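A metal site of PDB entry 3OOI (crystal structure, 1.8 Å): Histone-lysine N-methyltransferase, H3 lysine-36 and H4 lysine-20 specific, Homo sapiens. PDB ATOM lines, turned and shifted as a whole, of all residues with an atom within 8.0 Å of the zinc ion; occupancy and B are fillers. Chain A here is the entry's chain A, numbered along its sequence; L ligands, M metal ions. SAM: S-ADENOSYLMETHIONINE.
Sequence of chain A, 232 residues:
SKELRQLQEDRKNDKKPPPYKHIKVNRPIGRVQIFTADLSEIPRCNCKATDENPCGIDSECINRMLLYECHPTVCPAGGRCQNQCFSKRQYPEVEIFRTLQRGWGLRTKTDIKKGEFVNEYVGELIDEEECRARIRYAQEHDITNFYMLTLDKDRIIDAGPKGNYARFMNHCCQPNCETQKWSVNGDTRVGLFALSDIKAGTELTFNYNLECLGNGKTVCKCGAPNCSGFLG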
ATOM      1  N   ARG A 102      21.281  12.421  27.930  1.00  0.00           N
ATOM      2  CA  ARG A 102      21.658  12.981  26.611  1.00  0.00           C
ATOM      3  C   ARG A 102      21.779  11.863  25.564  1.00  0.00           C
ATOM      4  O   ARG A 102      22.615  11.917  24.645  1.00  0.00           O
ATOM      5  CB  ARG A 102      22.961  13.802  26.742  1.00  0.00           C
ATOM      6  CG  ARG A 102      22.815  15.036  27.678  1.00  0.00           C
ATOM      7  CD  ARG A 102      24.183  15.646  28.110  1.00  0.00           C
ATOM      8  NE  ARG A 102      24.941  14.666  28.880  1.00  0.00           N
ATOM      9  CZ  ARG A 102      26.055  14.080  28.461  1.00  0.00           C
ATOM     10  NH1 ARG A 102      26.605  14.424  27.299  1.00  0.00           N
ATOM     11  NH2 ARG A 102      26.649  13.143  29.208  1.00  0.00           N
ATOM     12  N   HIS A 171      26.397  18.060  23.054  1.00  0.00           N
ATOM     13  CA  HIS A 171      26.700  19.475  23.342  1.00  0.00           C
ATOM     14  C   HIS A 171      27.111  19.644  24.805  1.00  0.00           C
ATOM     15  O   HIS A 171      26.508  19.054  25.692  1.00  0.00           O
ATOM     16  CB  HIS A 171      25.461  20.365  23.093  1.00  0.00           C
ATOM     17  CG  HIS A 171      25.601  21.717  23.734  1.00  0.00           C
ATOM     18  ND1 HIS A 171      26.207  22.771  23.100  1.00  0.00           N
ATOM     19  CD2 HIS A 171      25.303  22.150  24.991  1.00  0.00           C
ATOM     20  CE1 HIS A 171      26.247  23.815  23.908  1.00  0.00           C
ATOM     21  NE2 HIS A 171      25.697  23.468  25.061  1.00  0.00           N
ATOM     22  N   CYS A 172      28.127  20.458  25.050  1.00  0.00           N
ATOM     23  CA  CYS A 172      28.482  20.855  26.404  1.00  0.00           C
ATOM     24  C   CYS A 172      28.813  22.338  26.411  1.00  0.00           C
ATOM     25  O   CYS A 172      29.448  22.835  25.466  1.00  0.00           O
ATOM     26  CB  CYS A 172      29.659  20.044  26.918  1.00  0.00           C
ATOM     27  SG  CYS A 172      30.045  20.330  28.661  1.00  0.00           S
ATOM     28  N   CYS A 173      28.362  23.026  27.452  1.00  0.00           N
ATOM     29  CA  CYS A 173      28.687  24.449  27.678  1.00  0.00           C
ATOM     30  C   CYS A 173      30.132  24.643  28.162  1.00  0.00           C
ATOM     31  O   CYS A 173      30.646  25.746  28.065  1.00  0.00           O
ATOM     32  CB  CYS A 173      27.682  25.074  28.652  1.00  0.00           C
ATOM     33  SG  CYS A 173      25.965  25.076  28.009  1.00  0.00           S
ATOM     34  N   GLN A 174      30.753  23.565  28.656  1.00  0.00           N
ATOM     35  CA  GLN A 174      32.211  23.519  28.950  1.00  0.00           C
ATOM     36  C   GLN A 174      32.873  22.375  28.165  1.00  0.00           C
ATOM     37  O   GLN A 174      33.349  21.389  28.750  1.00  0.00           O
ATOM     38  CB  GLN A 174      32.433  23.322  30.454  1.00  0.00           C
ATOM     39  CG  GLN A 174      32.482  24.628  31.192  1.00  0.00           C
ATOM     40  CD  GLN A 174      32.913  24.487  32.647  1.00  0.00           C
ATOM     41  OE1 GLN A 174      32.992  23.366  33.193  1.00  0.00           O
ATOM     42  NE2 GLN A 174      33.185  25.613  33.288  1.00  0.00           N
ATOM     43  N   ASN A 207      30.627  22.683  21.810  1.00  0.00           N
ATOM     44  CA  ASN A 207      29.572  23.643  21.960  1.00  0.00           C
ATOM     45  C   ASN A 207      28.877  23.764  20.603  1.00  0.00           C
ATOM     46  O   ASN A 207      29.471  24.184  19.612  1.00  0.00           O
ATOM     47  CB  ASN A 207      30.121  25.011  22.442  1.00  0.00           C
ATOM     48  CG  ASN A 207      29.022  25.991  22.821  1.00  0.00           C
ATOM     49  OD1 ASN A 207      27.955  26.007  22.224  1.00  0.00           O
ATOM     50  ND2 ASN A 207      29.283  26.808  23.854  1.00  0.00           N
ATOM     51  N   VAL A 219      16.321  22.240  26.189  1.00  0.00           N
ATOM     52  CA  VAL A 219      16.959  22.557  27.460  1.00  0.00           C
ATOM     53  C   VAL A 219      18.246  21.758  27.598  1.00  0.00           C
ATOM     54  O   VAL A 219      18.239  20.535  27.451  1.00  0.00           O
ATOM     55  CB  VAL A 219      16.030  22.256  28.676  1.00  0.00           C
ATOM     56  CG1 VAL A 219      16.775  22.481  29.997  1.00  0.00           C
ATOM     57  CG2 VAL A 219      14.762  23.137  28.613  1.00  0.00           C
ATOM     58  N   CYS A 220      19.341  22.447  27.898  1.00  0.00           N
ATOM     59  CA  CYS A 220      20.624  21.791  28.034  1.00  0.00           C
ATOM     60  C   CYS A 220      20.723  20.989  29.341  1.00  0.00           C
ATOM     61  O   CYS A 220      20.369  21.486  30.414  1.00  0.00           O
ATOM     62  CB  CYS A 220      21.757  22.802  27.984  1.00  0.00           C
ATOM     63  SG  CYS A 220      23.393  22.011  27.950  1.00  0.00           S
ATOM     64  N   LYS A 221      21.238  19.773  29.211  1.00  0.00           N
ATOM     65  CA  LYS A 221      21.444  18.890  30.360  1.00  0.00           C
ATOM     66  C   LYS A 221      22.932  18.585  30.552  1.00  0.00           C
ATOM     67  O   LYS A 221      23.292  17.556  31.128  1.00  0.00           O
ATOM     68  CB  LYS A 221      20.653  17.583  30.175  1.00  0.00           C
ATOM     69  CG  LYS A 221      19.139  17.762  29.939  1.00  0.00           C
ATOM     70  CD  LYS A 221      18.456  18.374  31.135  1.00  0.00           C
ATOM     71  CE  LYS A 221      16.994  18.685  30.830  1.00  0.00           C
ATOM     72  NZ  LYS A 221      16.410  19.447  31.968  1.00  0.00           N
ATOM     73  N   CYS A 222      23.794  19.495  30.093  1.00  0.00           N
ATOM     74  CA  CYS A 222      25.253  19.242  30.168  1.00  0.00           C
ATOM     75  C   CYS A 222      25.823  19.247  31.579  1.00  0.00           C
ATOM     76  O   CYS A 222      26.891  18.679  31.811  1.00  0.00           O
ATOM     77  CB  CYS A 222      26.052  20.200  29.282  1.00  0.00           C
ATOM     78  SG  CYS A 222      26.401  21.841  30.025  1.00  0.00           S
ATOM     79  N   GLY A 223      25.120  19.897  32.507  1.00  0.00           N
ATOM     80  CA  GLY A 223      25.518  19.909  33.924  1.00  0.00           C
ATOM     81  C   GLY A 223      26.714  20.778  34.293  1.00  0.00           C
ATOM     82  O   GLY A 223      27.139  20.752  35.453  1.00  0.00           O
ATOM     83  N   ALA A 224      27.254  21.533  33.342  1.00  0.00           N
ATOM     84  CA  ALA A 224      28.371  22.435  33.615  1.00  0.00           C
ATOM     85  C   ALA A 224      27.954  23.572  34.543  1.00  0.00           C
ATOM     86  O   ALA A 224      26.787  23.992  34.544  1.00  0.00           O
ATOM     87  CB  ALA A 224      28.971  22.975  32.308  1.00  0.00           C
ATOM     88  N   PRO A 225      28.898  24.086  35.368  1.00  0.00           N
ATOM     89  CA  PRO A 225      28.536  25.181  36.269  1.00  0.00           C
ATOM     90  C   PRO A 225      28.188  26.482  35.537  1.00  0.00           C
ATOM     91  O   PRO A 225      27.457  27.316  36.080  1.00  0.00           O
ATOM     92  CB  PRO A 225      29.781  25.360  37.143  1.00  0.00           C
ATOM     93  CG  PRO A 225      30.904  24.754  36.379  1.00  0.00           C
ATOM     94  CD  PRO A 225      30.289  23.623  35.579  1.00  0.00           C
ATOM     95  N   ASN A 226      28.690  26.632  34.313  1.00  0.00           N
ATOM     96  CA  ASN A 226      28.400  27.801  33.482  1.00  0.00           C
ATOM     97  C   ASN A 226      27.302  27.541  32.433  1.00  0.00           C
ATOM     98  O   ASN A 226      27.217  28.249  31.416  1.00  0.00           O
ATOM     99  CB  ASN A 226      29.679  28.265  32.779  1.00  0.00           C
ATOM    100  CG  ASN A 226      30.118  27.323  31.672  1.00  0.00           C
ATOM    101  OD1 ASN A 226      29.888  26.121  31.731  1.00  0.00           O
ATOM    102  ND2 ASN A 226      30.743  27.878  30.631  1.00  0.00           N
ATOM    103  N   CYS A 227      26.460  26.537  32.667  1.00  0.00           N
ATOM    104  CA  CYS A 227      25.475  26.128  31.650  1.00  0.00           C
ATOM    105  C   CYS A 227      24.552  27.283  31.239  1.00  0.00           C
ATOM    106  O   CYS A 227      23.942  27.943  32.090  1.00  0.00           O
ATOM    107  CB  CYS A 227      24.661  24.932  32.107  1.00  0.00           C
ATOM    108  SG  CYS A 227      23.484  24.324  30.885  1.00  0.00           S
ATOM    109  N   SER A 228      24.447  27.508  29.933  1.00  0.00           N
ATOM    110  CA  SER A 228      23.569  28.564  29.394  1.00  0.00           C
ATOM    111  C   SER A 228      22.092  28.185  29.486  1.00  0.00           C
ATOM    112  O   SER A 228      21.219  29.060  29.392  1.00  0.00           O
ATOM    113  CB  SER A 228      23.897  28.773  27.917  1.00  0.00           C
ATOM    114  OG  SER A 228      23.470  27.625  27.197  1.00  0.00           O
ATOM    115  N   GLY A 229      21.816  26.893  29.614  1.00  0.00           N
ATOM    116  CA  GLY A 229      20.447  26.377  29.613  1.00  0.00           C
ATOM    117  C   GLY A 229      19.946  25.935  28.249  1.00  0.00           C
ATOM    118  O   GLY A 229      18.849  25.388  28.110  1.00  0.00           O
ATOM    119  N   PHE A 230      20.759  26.198  27.217  1.00  0.00           N
ATOM    120  CA  PHE A 230      20.401  25.838  25.844  1.00  0.00           C
ATOM    121  C   PHE A 230      21.612  25.255  25.102  1.00  0.00           C
ATOM    122  O   PHE A 230      22.739  25.280  25.633  1.00  0.00           O
ATOM    123  CB  PHE A 230      19.782  27.033  25.106  1.00  0.00           C
ATOM    124  CG  PHE A 230      20.626  28.296  25.130  1.00  0.00           C
ATOM    125  CD1 PHE A 230      21.601  28.523  24.150  1.00  0.00           C
ATOM    126  CD2 PHE A 230      20.402  29.291  26.085  1.00  0.00           C
ATOM    127  CE1 PHE A 230      22.363  29.709  24.145  1.00  0.00           C
ATOM    128  CE2 PHE A 230      21.164  30.470  26.092  1.00  0.00           C
ATOM    129  CZ  PHE A 230      22.140  30.685  25.105  1.00  0.00           C
ATOM    130  N   LEU A 231      21.393  24.721  23.903  1.00  0.00           N
ATOM    131  CA  LEU A 231      22.499  24.054  23.194  1.00  0.00           C
ATOM    132  C   LEU A 231      23.357  25.067  22.433  1.00  0.00           C
ATOM    133  O   LEU A 231      23.454  25.027  21.204  1.00  0.00           O
ATOM    134  CB  LEU A 231      21.991  22.908  22.292  1.00  0.00           C
ATOM    135  CG  LEU A 231      21.113  21.838  22.951  1.00  0.00           C
ATOM    136  CD1 LEU A 231      20.957  20.624  21.989  1.00  0.00           C
ATOM    137  CD2 LEU A 231      21.567  21.401  24.323  1.00  0.00           C
ATOM    138  N   GLY A 232      23.965  25.981  23.191  1.00  0.00           N
ATOM    139  CA  GLY A 232      24.809  27.037  22.614  1.00  0.00           C
ATOM    140  C   GLY A 232      25.359  27.976  23.671  1.00  0.00           C
ATOM    141  O   GLY A 232      25.338  27.656  24.877  1.00  0.00           O
ATOM    142  OXT GLY A 232      25.855  29.067  23.359  1.00  0.00           O
HETATM  143  N   SAM L   1      22.641  12.167  21.942  1.00  0.00           N
HETATM  144  CA  SAM L   1      22.601  11.902  20.467  1.00  0.00           C
HETATM  145  C   SAM L   1      22.097  10.482  20.186  1.00  0.00           C
HETATM  146  O   SAM L   1      21.578   9.754  21.070  1.00  0.00           O
HETATM  147  OXT SAM L   1      22.189  10.032  19.052  1.00  0.00           O
HETATM  148  CB  SAM L   1      23.963  12.212  19.826  1.00  0.00           C
HETATM  149  CG  SAM L   1      24.152  13.731  19.598  1.00  0.00           C
HETATM  150  SD  SAM L   1      23.043  14.356  18.288  1.00  0.00           S
HETATM  151  CE  SAM L   1      24.161  15.258  17.191  1.00  0.00           C
HETATM  152  C5' SAM L   1      22.244  15.775  19.060  1.00  0.00           C
HETATM  153  C4' SAM L   1      21.083  15.436  19.980  1.00  0.00           C
HETATM  154  O4' SAM L   1      21.516  14.951  21.248  1.00  0.00           O
HETATM  155  C3' SAM L   1      20.267  16.671  20.248  1.00  0.00           C
HETATM  156  O3' SAM L   1      19.284  16.866  19.254  1.00  0.00           O
HETATM  157  C2' SAM L   1      19.708  16.409  21.627  1.00  0.00           C
HETATM  158  O2' SAM L   1      18.532  15.600  21.545  1.00  0.00           O
HETATM  159  C1' SAM L   1      20.798  15.586  22.292  1.00  0.00           C
HETATM  160  N9  SAM L   1      21.734  16.412  23.085  1.00  0.00           N
HETATM  161  C8  SAM L   1      23.069  16.593  22.822  1.00  0.00           C
HETATM  162  N7  SAM L   1      23.608  17.376  23.790  1.00  0.00           N
HETATM  163  C5  SAM L   1      22.619  17.663  24.680  1.00  0.00           C
HETATM  164  C6  SAM L   1      22.618  18.402  25.866  1.00  0.00           C
HETATM  165  N6  SAM L   1      23.703  19.013  26.317  1.00  0.00           N
HETATM  166  N1  SAM L   1      21.454  18.525  26.564  1.00  0.00           N
HETATM  167  C2  SAM L   1      20.298  17.912  26.128  1.00  0.00           C
HETATM  168  N3  SAM L   1      20.288  17.166  24.963  1.00  0.00           N
HETATM  169  C4  SAM L   1      21.452  17.043  24.265  1.00  0.00           C
HETATM  170 ZN    ZN M   1      24.802  23.328  29.208  1.00  0.00          ZN
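The backbone NH of His 171 sits at hydrogen-bond distance from a nitrogen (N7) of the ligand, 3.0 Å away.
A nitrogen (N) of the ligand lies within hydrogen-bond range of the backbone carbonyl oxygen of Arg 102 (2.7 Å).
N6 of the ligand sits close to SG of Cys 220 (3.4 Å).
N of Lys 221 lies within hydrogen-bond range of N1 of the ligand (2.9 Å).
The backbone carbonyl oxygen (O) of His 171 lies within hydrogen-bond range of a nitrogen (N6) of the ligand (2.9 Å).
The zinc ion is bound by SG of Cys 220, 2.3 Å away.
The side-chain sulfur (SG) of Cys 222 is bound to the zinc ion (2.3 Å).
SG of Cys 227 is bound to the zinc ion, at 2.4 Å.
SG of Cys 173 binds the zinc ion, at 2.4 Å.
Four residues have an atom within 4 Å of the zinc ion: Cys 173, Cys 220, Cys 222 and Cys 227.
Along chain A the residues within 4 Å of the zinc ion span positions 173 to 227.
The side-chain sulfur (SG) of Cys 227 sits close to the backbone NH (N) of Gly 229 (3.3 Å).
The backbone NH (N) of Cys 220 lies within hydrogen-bond range of the backbone carbonyl oxygen (O) of Gly 229.
The side-chain sulfur of Cys 173 lies close to the backbone NH of Ser 228, 3.5 Å away.
The side-chain sulfur of Cys 173 sits close to a ring nitrogen (NE2) of His 171, 3.4 Å away.
The backbone NH (N) of Ala 224 lies close to the side-chain sulfur (SG) of Cys 222 (3.4 Å).
ND2 of Asn 226 lies within hydrogen-bond range of O of Cys 173.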
